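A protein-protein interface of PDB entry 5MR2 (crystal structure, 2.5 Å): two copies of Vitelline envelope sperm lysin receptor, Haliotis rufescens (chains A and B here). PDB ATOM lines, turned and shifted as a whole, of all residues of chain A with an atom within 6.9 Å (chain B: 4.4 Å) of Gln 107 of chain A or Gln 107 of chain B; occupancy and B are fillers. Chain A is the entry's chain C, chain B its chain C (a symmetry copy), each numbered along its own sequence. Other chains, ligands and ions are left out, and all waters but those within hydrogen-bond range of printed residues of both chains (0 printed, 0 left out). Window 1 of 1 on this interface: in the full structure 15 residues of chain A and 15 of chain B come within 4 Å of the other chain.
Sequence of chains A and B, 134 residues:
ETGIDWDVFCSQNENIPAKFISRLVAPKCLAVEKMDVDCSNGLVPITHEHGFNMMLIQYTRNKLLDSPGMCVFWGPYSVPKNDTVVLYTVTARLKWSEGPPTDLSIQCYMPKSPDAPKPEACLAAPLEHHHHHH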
ATOM      1  N   TRP A   6      25.092  22.523  32.535  1.00  0.00           N
ATOM      2  CA  TRP A   6      24.001  23.466  32.789  1.00  0.00           C
ATOM      3  C   TRP A   6      22.651  22.767  32.863  1.00  0.00           C
ATOM      4  O   TRP A   6      22.499  21.613  32.446  1.00  0.00           O
ATOM      5  CB  TRP A   6      23.937  24.556  31.707  1.00  0.00           C
ATOM      6  CG  TRP A   6      23.649  24.032  30.335  1.00  0.00           C
ATOM      7  CD1 TRP A   6      24.466  23.257  29.563  1.00  0.00           C
ATOM      8  CD2 TRP A   6      22.465  24.264  29.556  1.00  0.00           C
ATOM      9  NE1 TRP A   6      23.859  22.971  28.368  1.00  0.00           N
ATOM     10  CE2 TRP A   6      22.627  23.580  28.337  1.00  0.00           C
ATOM     11  CE3 TRP A   6      21.289  24.980  29.770  1.00  0.00           C
ATOM     12  CZ2 TRP A   6      21.657  23.606  27.329  1.00  0.00           C
ATOM     13  CZ3 TRP A   6      20.327  24.990  28.776  1.00  0.00           C
ATOM     14  CH2 TRP A   6      20.519  24.311  27.573  1.00  0.00           C
ATOM     15  N   VAL A   8      18.136  24.220  33.488  1.00  0.00           N
ATOM     16  CA  VAL A   8      17.162  25.288  33.675  1.00  0.00           C
ATOM     17  C   VAL A   8      16.175  24.823  34.725  1.00  0.00           C
ATOM     18  O   VAL A   8      15.681  23.696  34.648  1.00  0.00           O
ATOM     19  CB  VAL A   8      16.396  25.613  32.377  1.00  0.00           C
ATOM     20  CG1 VAL A   8      15.469  26.788  32.620  1.00  0.00           C
ATOM     21  CG2 VAL A   8      17.334  25.862  31.211  1.00  0.00           C
ATOM     22  N   CYS A  10      12.670  25.793  35.903  1.00  0.00           N
ATOM     23  CA  CYS A  10      11.503  26.579  35.577  1.00  0.00           C
ATOM     24  C   CYS A  10      10.632  26.743  36.813  1.00  0.00           C
ATOM     25  O   CYS A  10      10.666  25.930  37.736  1.00  0.00           O
ATOM     26  CB  CYS A  10      10.740  25.909  34.437  1.00  0.00           C
ATOM     27  SG  CYS A  10      11.746  25.667  32.910  1.00  0.00           S
ATOM     28  N   TYR A  59       9.517  35.937  33.396  1.00  0.00           N
ATOM     29  CA  TYR A  59       8.465  35.692  32.430  1.00  0.00           C
ATOM     30  C   TYR A  59       7.745  36.972  32.031  1.00  0.00           C
ATOM     31  O   TYR A  59       7.202  37.044  30.922  1.00  0.00           O
ATOM     32  CB  TYR A  59       7.460  34.698  32.991  1.00  0.00           C
ATOM     33  CG  TYR A  59       8.000  33.330  33.282  1.00  0.00           C
ATOM     34  CD1 TYR A  59       8.557  33.025  34.511  1.00  0.00           C
ATOM     35  CD2 TYR A  59       7.934  32.332  32.334  1.00  0.00           C
ATOM     36  CE1 TYR A  59       9.028  31.756  34.787  1.00  0.00           C
ATOM     37  CE2 TYR A  59       8.410  31.062  32.591  1.00  0.00           C
ATOM     38  CZ  TYR A  59       8.951  30.775  33.823  1.00  0.00           C
ATOM     39  OH  TYR A  59       9.422  29.505  34.083  1.00  0.00           O
ATOM     40  N   PHE A  73      12.044  36.384  29.170  1.00  0.00           N
ATOM     41  CA  PHE A  73      11.803  35.331  28.200  1.00  0.00           C
ATOM     42  C   PHE A  73      11.149  35.891  26.946  1.00  0.00           C
ATOM     43  O   PHE A  73      10.357  36.835  27.004  1.00  0.00           O
ATOM     44  CB  PHE A  73      10.867  34.264  28.769  1.00  0.00           C
ATOM     45  CG  PHE A  73      11.539  33.184  29.557  1.00  0.00           C
ATOM     46  CD1 PHE A  73      12.445  32.332  28.957  1.00  0.00           C
ATOM     47  CD2 PHE A  73      11.195  32.968  30.876  1.00  0.00           C
ATOM     48  CE1 PHE A  73      13.031  31.321  29.668  1.00  0.00           C
ATOM     49  CE2 PHE A  73      11.781  31.949  31.597  1.00  0.00           C
ATOM     50  CZ  PHE A  73      12.700  31.129  30.993  1.00  0.00           C
ATOM     51  N   SER A  78       2.581  29.209  21.396  1.00  0.00           N
ATOM     52  CA  SER A  78       1.778  28.007  21.253  1.00  0.00           C
ATOM     53  C   SER A  78       2.595  26.888  20.613  1.00  0.00           C
ATOM     54  O   SER A  78       3.533  27.133  19.843  1.00  0.00           O
ATOM     55  CB  SER A  78       0.533  28.308  20.439  1.00  0.00           C
ATOM     56  OG  SER A  78      -0.251  29.248  21.152  1.00  0.00           O
ATOM     57  N   VAL A  79       2.224  25.653  20.949  1.00  0.00           N
ATOM     58  CA  VAL A  79       2.935  24.430  20.566  1.00  0.00           C
ATOM     59  C   VAL A  79       1.988  23.565  19.736  1.00  0.00           C
ATOM     60  O   VAL A  79       0.787  23.533  20.035  1.00  0.00           O
ATOM     61  CB  VAL A  79       3.472  23.721  21.825  1.00  0.00           C
ATOM     62  CG1 VAL A  79       3.930  22.295  21.553  1.00  0.00           C
ATOM     63  CG2 VAL A  79       4.646  24.527  22.381  1.00  0.00           C
ATOM     64  N   PRO A  80       2.454  22.874  18.683  1.00  0.00           N
ATOM     65  CA  PRO A  80       1.492  22.228  17.771  1.00  0.00           C
ATOM     66  C   PRO A  80       0.614  21.160  18.414  1.00  0.00           C
ATOM     67  O   PRO A  80      -0.584  21.085  18.105  1.00  0.00           O
ATOM     68  CB  PRO A  80       2.394  21.654  16.666  1.00  0.00           C
ATOM     69  CG  PRO A  80       3.730  21.569  17.248  1.00  0.00           C
ATOM     70  CD  PRO A  80       3.837  22.716  18.198  1.00  0.00           C
ATOM     71  N   LEU A  87       4.986  28.123  25.720  1.00  0.00           N
ATOM     72  CA  LEU A  87       6.434  28.049  25.817  1.00  0.00           C
ATOM     73  C   LEU A  87       6.996  29.431  26.053  1.00  0.00           C
ATOM     74  O   LEU A  87       6.604  30.389  25.383  1.00  0.00           O
ATOM     75  CB  LEU A  87       7.053  27.470  24.547  1.00  0.00           C
ATOM     76  CG  LEU A  87       8.577  27.536  24.464  1.00  0.00           C
ATOM     77  CD1 LEU A  87       9.222  26.526  25.444  1.00  0.00           C
ATOM     78  CD2 LEU A  87       9.072  27.304  23.062  1.00  0.00           C
ATOM     79  N   TYR A  88       7.902  29.532  27.014  1.00  0.00           N
ATOM     80  CA  TYR A  88       8.790  30.674  27.121  1.00  0.00           C
ATOM     81  C   TYR A  88      10.206  30.204  26.853  1.00  0.00           C
ATOM     82  O   TYR A  88      10.572  29.079  27.209  1.00  0.00           O
ATOM     83  CB  TYR A  88       8.703  31.303  28.491  1.00  0.00           C
ATOM     84  CG  TYR A  88       7.351  31.892  28.838  1.00  0.00           C
ATOM     85  CD1 TYR A  88       6.334  31.092  29.339  1.00  0.00           C
ATOM     86  CD2 TYR A  88       7.116  33.260  28.701  1.00  0.00           C
ATOM     87  CE1 TYR A  88       5.123  31.637  29.687  1.00  0.00           C
ATOM     88  CE2 TYR A  88       5.918  33.808  29.041  1.00  0.00           C
ATOM     89  CZ  TYR A  88       4.923  33.000  29.532  1.00  0.00           C
ATOM     90  OH  TYR A  88       3.726  33.581  29.870  1.00  0.00           O
ATOM     91  N   THR A  89      11.005  31.055  26.217  1.00  0.00           N
ATOM     92  CA  THR A  89      12.346  30.619  25.848  1.00  0.00           C
ATOM     93  C   THR A  89      13.269  31.818  25.676  1.00  0.00           C
ATOM     94  O   THR A  89      12.821  32.965  25.600  1.00  0.00           O
ATOM     95  CB  THR A  89      12.319  29.716  24.593  1.00  0.00           C
ATOM     96  OG1 THR A  89      13.658  29.347  24.222  1.00  0.00           O
ATOM     97  CG2 THR A  89      11.610  30.362  23.439  1.00  0.00           C
ATOM     98  N   VAL A  90      14.573  31.534  25.752  1.00  0.00           N
ATOM     99  CA  VAL A  90      15.648  32.414  25.291  1.00  0.00           C
ATOM    100  C   VAL A  90      16.758  31.501  24.780  1.00  0.00           C
ATOM    101  O   VAL A  90      16.672  30.274  24.900  1.00  0.00           O
ATOM    102  CB  VAL A  90      16.192  33.359  26.386  1.00  0.00           C
ATOM    103  CG1 VAL A  90      15.081  34.181  27.021  1.00  0.00           C
ATOM    104  CG2 VAL A  90      17.008  32.581  27.432  1.00  0.00           C
ATOM    105  N   SER A 105      19.583  26.319  24.075  1.00  0.00           N
ATOM    106  CA  SER A 105      18.155  26.594  24.035  1.00  0.00           C
ATOM    107  C   SER A 105      17.604  26.404  25.440  1.00  0.00           C
ATOM    108  O   SER A 105      17.737  25.322  26.015  1.00  0.00           O
ATOM    109  CB  SER A 105      17.472  25.658  23.034  1.00  0.00           C
ATOM    110  OG  SER A 105      16.063  25.713  23.116  1.00  0.00           O
ATOM    111  N   ILE A 106      17.000  27.447  25.989  1.00  0.00           N
ATOM    112  CA  ILE A 106      16.526  27.476  27.367  1.00  0.00           C
ATOM    113  C   ILE A 106      15.009  27.587  27.329  1.00  0.00           C
ATOM    114  O   ILE A 106      14.470  28.671  27.095  1.00  0.00           O
ATOM    115  CB  ILE A 106      17.153  28.653  28.135  1.00  0.00           C
ATOM    116  CG1 ILE A 106      18.656  28.450  28.293  1.00  0.00           C
ATOM    117  CG2 ILE A 106      16.527  28.868  29.497  1.00  0.00           C
ATOM    118  CD1 ILE A 106      19.382  29.729  28.518  1.00  0.00           C
ATOM    119  N   GLN A 107      14.310  26.506  27.656  1.00  0.00           N
ATOM    120  CA  GLN A 107      12.873  26.432  27.441  1.00  0.00           C
ATOM    121  C   GLN A 107      12.155  26.202  28.763  1.00  0.00           C
ATOM    122  O   GLN A 107      12.554  25.339  29.549  1.00  0.00           O
ATOM    123  CB  GLN A 107      12.537  25.312  26.444  1.00  0.00           C
ATOM    124  CG  GLN A 107      13.140  25.526  25.054  1.00  0.00           C
ATOM    125  CD  GLN A 107      12.728  24.468  24.049  1.00  0.00           C
ATOM    126  OE1 GLN A 107      11.577  24.405  23.619  1.00  0.00           O
ATOM    127  NE2 GLN A 107      13.672  23.626  23.669  1.00  0.00           N
ATOM    128  N   CYS A 108      11.082  26.967  28.990  1.00  0.00           N
ATOM    129  CA  CYS A 108      10.198  26.778  30.133  1.00  0.00           C
ATOM    130  C   CYS A 108       8.743  26.837  29.685  1.00  0.00           C
ATOM    131  O   CYS A 108       8.294  27.857  29.148  1.00  0.00           O
ATOM    132  CB  CYS A 108      10.460  27.830  31.210  1.00  0.00           C
ATOM    133  SG  CYS A 108      11.986  27.537  32.095  1.00  0.00           S
ATOM    134  N   TYR A 109       8.009  25.761  29.963  1.00  0.00           N
ATOM    135  CA  TYR A 109       6.580  25.685  29.721  1.00  0.00           C
ATOM    136  C   TYR A 109       5.807  26.132  30.952  1.00  0.00           C
ATOM    137  O   TYR A 109       6.211  25.864  32.084  1.00  0.00           O
ATOM    138  CB  TYR A 109       6.185  24.262  29.348  1.00  0.00           C
ATOM    139  CG  TYR A 109       6.700  23.849  28.004  1.00  0.00           C
ATOM    140  CD1 TYR A 109       7.982  23.356  27.851  1.00  0.00           C
ATOM    141  CD2 TYR A 109       5.905  23.968  26.876  1.00  0.00           C
ATOM    142  CE1 TYR A 109       8.451  22.981  26.606  1.00  0.00           C
ATOM    143  CE2 TYR A 109       6.366  23.604  25.639  1.00  0.00           C
ATOM    144  CZ  TYR A 109       7.635  23.109  25.509  1.00  0.00           C
ATOM    145  OH  TYR A 109       8.084  22.743  24.271  1.00  0.00           O
ATOM    146  N   CYS B  10       8.669  17.272  10.815  1.00  0.00           N
ATOM    147  CA  CYS B  10      10.112  17.337  10.808  1.00  0.00           C
ATOM    148  C   CYS B  10      10.672  16.215   9.947  1.00  0.00           C
ATOM    149  O   CYS B  10      10.039  15.180   9.748  1.00  0.00           O
ATOM    150  CB  CYS B  10      10.632  17.258  12.241  1.00  0.00           C
ATOM    151  SG  CYS B  10       9.977  18.584  13.344  1.00  0.00           S
ATOM    152  N   LEU B  87      18.324  21.018  18.619  1.00  0.00           N
ATOM    153  CA  LEU B  87      17.060  21.661  18.300  1.00  0.00           C
ATOM    154  C   LEU B  87      17.257  22.618  17.149  1.00  0.00           C
ATOM    155  O   LEU B  87      18.212  23.397  17.139  1.00  0.00           O
ATOM    156  CB  LEU B  87      16.503  22.429  19.497  1.00  0.00           C
ATOM    157  CG  LEU B  87      15.284  23.305  19.210  1.00  0.00           C
ATOM    158  CD1 LEU B  87      14.028  22.432  18.968  1.00  0.00           C
ATOM    159  CD2 LEU B  87      15.034  24.296  20.316  1.00  0.00           C
ATOM    160  N   TYR B  88      16.361  22.548  16.176  1.00  0.00           N
ATOM    161  CA  TYR B  88      16.188  23.611  15.206  1.00  0.00           C
ATOM    162  C   TYR B  88      14.820  24.231  15.416  1.00  0.00           C
ATOM    163  O   TYR B  88      13.864  23.535  15.771  1.00  0.00           O
ATOM    164  CB  TYR B  88      16.308  23.085  13.796  1.00  0.00           C
ATOM    165  CG  TYR B  88      17.667  22.520  13.439  1.00  0.00           C
ATOM    166  CD1 TYR B  88      18.001  21.212  13.763  1.00  0.00           C
ATOM    167  CD2 TYR B  88      18.596  23.290  12.740  1.00  0.00           C
ATOM    168  CE1 TYR B  88      19.221  20.693  13.405  1.00  0.00           C
ATOM    169  CE2 TYR B  88      19.808  22.784  12.383  1.00  0.00           C
ATOM    170  CZ  TYR B  88      20.121  21.490  12.715  1.00  0.00           C
ATOM    171  OH  TYR B  88      21.349  21.005  12.339  1.00  0.00           O
ATOM    172  N   THR B  89      14.721  25.541  15.205  1.00  0.00           N
ATOM    173  CA  THR B  89      13.454  26.204  15.485  1.00  0.00           C
ATOM    174  C   THR B  89      13.339  27.493  14.683  1.00  0.00           C
ATOM    175  O   THR B  89      14.319  27.986  14.118  1.00  0.00           O
ATOM    176  CB  THR B  89      13.265  26.439  17.002  1.00  0.00           C
ATOM    177  OG1 THR B  89      12.034  27.142  17.242  1.00  0.00           O
ATOM    178  CG2 THR B  89      14.421  27.172  17.616  1.00  0.00           C
ATOM    179  N   SER B 105       5.569  28.503  18.042  1.00  0.00           N
ATOM    180  CA  SER B 105       6.907  27.954  18.190  1.00  0.00           C
ATOM    181  C   SER B 105       6.985  26.684  17.355  1.00  0.00           C
ATOM    182  O   SER B 105       6.200  25.757  17.566  1.00  0.00           O
ATOM    183  CB  SER B 105       7.196  27.673  19.666  1.00  0.00           C
ATOM    184  OG  SER B 105       8.382  26.928  19.854  1.00  0.00           O
ATOM    185  N   ILE B 106       7.915  26.646  16.413  1.00  0.00           N
ATOM    186  CA  ILE B 106       8.047  25.561  15.448  1.00  0.00           C
ATOM    187  C   ILE B 106       9.375  24.868  15.714  1.00  0.00           C
ATOM    188  O   ILE B 106      10.430  25.375  15.326  1.00  0.00           O
ATOM    189  CB  ILE B 106       7.977  26.101  14.008  1.00  0.00           C
ATOM    190  CG1 ILE B 106       6.588  26.657  13.712  1.00  0.00           C
ATOM    191  CG2 ILE B 106       8.334  25.057  12.971  1.00  0.00           C
ATOM    192  CD1 ILE B 106       6.597  27.646  12.599  1.00  0.00           C
ATOM    193  N   GLN B 107       9.335  23.668  16.280  1.00  0.00           N
ATOM    194  CA  GLN B 107      10.536  23.017  16.779  1.00  0.00           C
ATOM    195  C   GLN B 107      10.749  21.689  16.066  1.00  0.00           C
ATOM    196  O   GLN B 107       9.813  20.897  15.928  1.00  0.00           O
ATOM    197  CB  GLN B 107      10.439  22.804  18.297  1.00  0.00           C
ATOM    198  CG  GLN B 107      10.328  24.105  19.094  1.00  0.00           C
ATOM    199  CD  GLN B 107      10.329  23.894  20.595  1.00  0.00           C
ATOM    200  OE1 GLN B 107      11.342  23.531  21.193  1.00  0.00           O
ATOM    201  NE2 GLN B 107       9.185  24.121  21.217  1.00  0.00           N
ATOM    202  N   CYS B 108      11.991  21.445  15.635  1.00  0.00           N
ATOM    203  CA  CYS B 108      12.399  20.167  15.066  1.00  0.00           C
ATOM    204  C   CYS B 108      13.732  19.731  15.662  1.00  0.00           C
ATOM    205  O   CYS B 108      14.740  20.434  15.524  1.00  0.00           O
ATOM    206  CB  CYS B 108      12.506  20.253  13.545  1.00  0.00           C
ATOM    207  SG  CYS B 108      10.906  20.316  12.750  1.00  0.00           S
ATOM    208  N   TYR B 109      13.732  18.545  16.269  1.00  0.00           N
ATOM    209  CA  TYR B 109      14.932  17.914  16.788  1.00  0.00           C
ATOM    210  C   TYR B 109      15.558  17.014  15.735  1.00  0.00           C
ATOM    211  O   TYR B 109      14.855  16.360  14.964  1.00  0.00           O
ATOM    212  CB  TYR B 109      14.603  17.104  18.035  1.00  0.00           C
ATOM    213  CG  TYR B 109      14.232  17.963  19.204  1.00  0.00           C
ATOM    214  CD1 TYR B 109      12.941  18.428  19.368  1.00  0.00           C
ATOM    215  CD2 TYR B 109      15.184  18.325  20.144  1.00  0.00           C
ATOM    216  CE1 TYR B 109      12.608  19.223  20.449  1.00  0.00           C
ATOM    217  CE2 TYR B 109      14.861  19.117  21.213  1.00  0.00           C
ATOM    218  CZ  TYR B 109      13.576  19.560  21.364  1.00  0.00           C
ATOM    219  OH  TYR B 109      13.262  20.346  22.438  1.00  0.00           O
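The side-chain amide oxygen (OE1) of Gln 107 of chain A sits close to the side-chain amide oxygen (OE1) of Gln 107 of chain B, at 2.6 Å. O of Ser 78 of chain A sits at hydrogen-bond distance from N of Ser 105 of chain B, 3.0 Å away.
The side-chain amide nitrogen (NE2) of Gln 107 of chain B is in hydrogen-bond range of the side-chain hydroxyl (OG) of Ser 105 of chain B (3.2 Å). The side-chain sulfur (SG) of Cys 10 of chain B forms a disulfide with the side-chain sulfur (SG) of Cys 108 of chain B (2.1 Å). The side-chain amide nitrogen of Gln 107 of chain A lies within hydrogen-bond range of the side-chain hydroxyl of Ser 105 of chain A, at 3.2 Å. SG of Cys 10 of chain A forms a disulfide with SG of Cys 108 of chain A.
Among the printed residues, pairs that only touch across the chains: Ser 105 of chain A with Leu 87 of chain B (3.3 Å), Leu 87 of chain A with Ser 105 of chain B (3.3 Å), Tyr 109 of chain A with Gln 107 of chain B (3.5 Å), Gln 107 of chain A with Tyr 109 of chain B (3.5 Å), Gln 107 of chain A with Leu 87 of chain B (3.7 Å), Leu 87 of chain A with Gln 107 of chain B (3.7 Å) and Pro 80 of chain A with Ser 105 of chain B (3.9 Å).
Gln 107 of chain A touches just these residues of chain B: Leu 87 (3.7 Å), Gln 107 (2.6 Å) and Tyr 109 (3.5 Å). Printed residues of chain B within 4 Å of Tyr 109 of chain A: Gln 107. Printed residues of chain A within 4 Å of Leu 87 of chain B: Ser 105 and Gln 107. Gln 107 of chain B touches three residues of chain A. The nearest printed residue of chain B that does not touch Leu 87 of chain A is Thr 89 of chain B (6.5 Å).
Hydrophobic or aromatic side chains of chain B that line the printed part of chain A: Leu 87 and Tyr 109. Along chain B the printed residues that touch a printed residue of chain A span positions 87 to 109. Hydrophobic or aromatic side chains of chain A that line the printed part of chain B: Pro 80, Leu 87 and Tyr 109.
Leu 87 of chain A touches Ser 105 of chain B, and with the chains exchanged Ser 105 of chain A touches Leu 87 of chain B. Leu 87 of chain A touches Gln 107 of chain B, and with the chains exchanged Gln 107 of chain A touches Leu 87 of chain B. Gln 107 of chain A touches its own counterpart, Gln 107 of chain B. Gln 107 of chain A touches Tyr 109 of chain B, and with the chains exchanged Tyr 109 of chain A touches Gln 107 of chain B.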
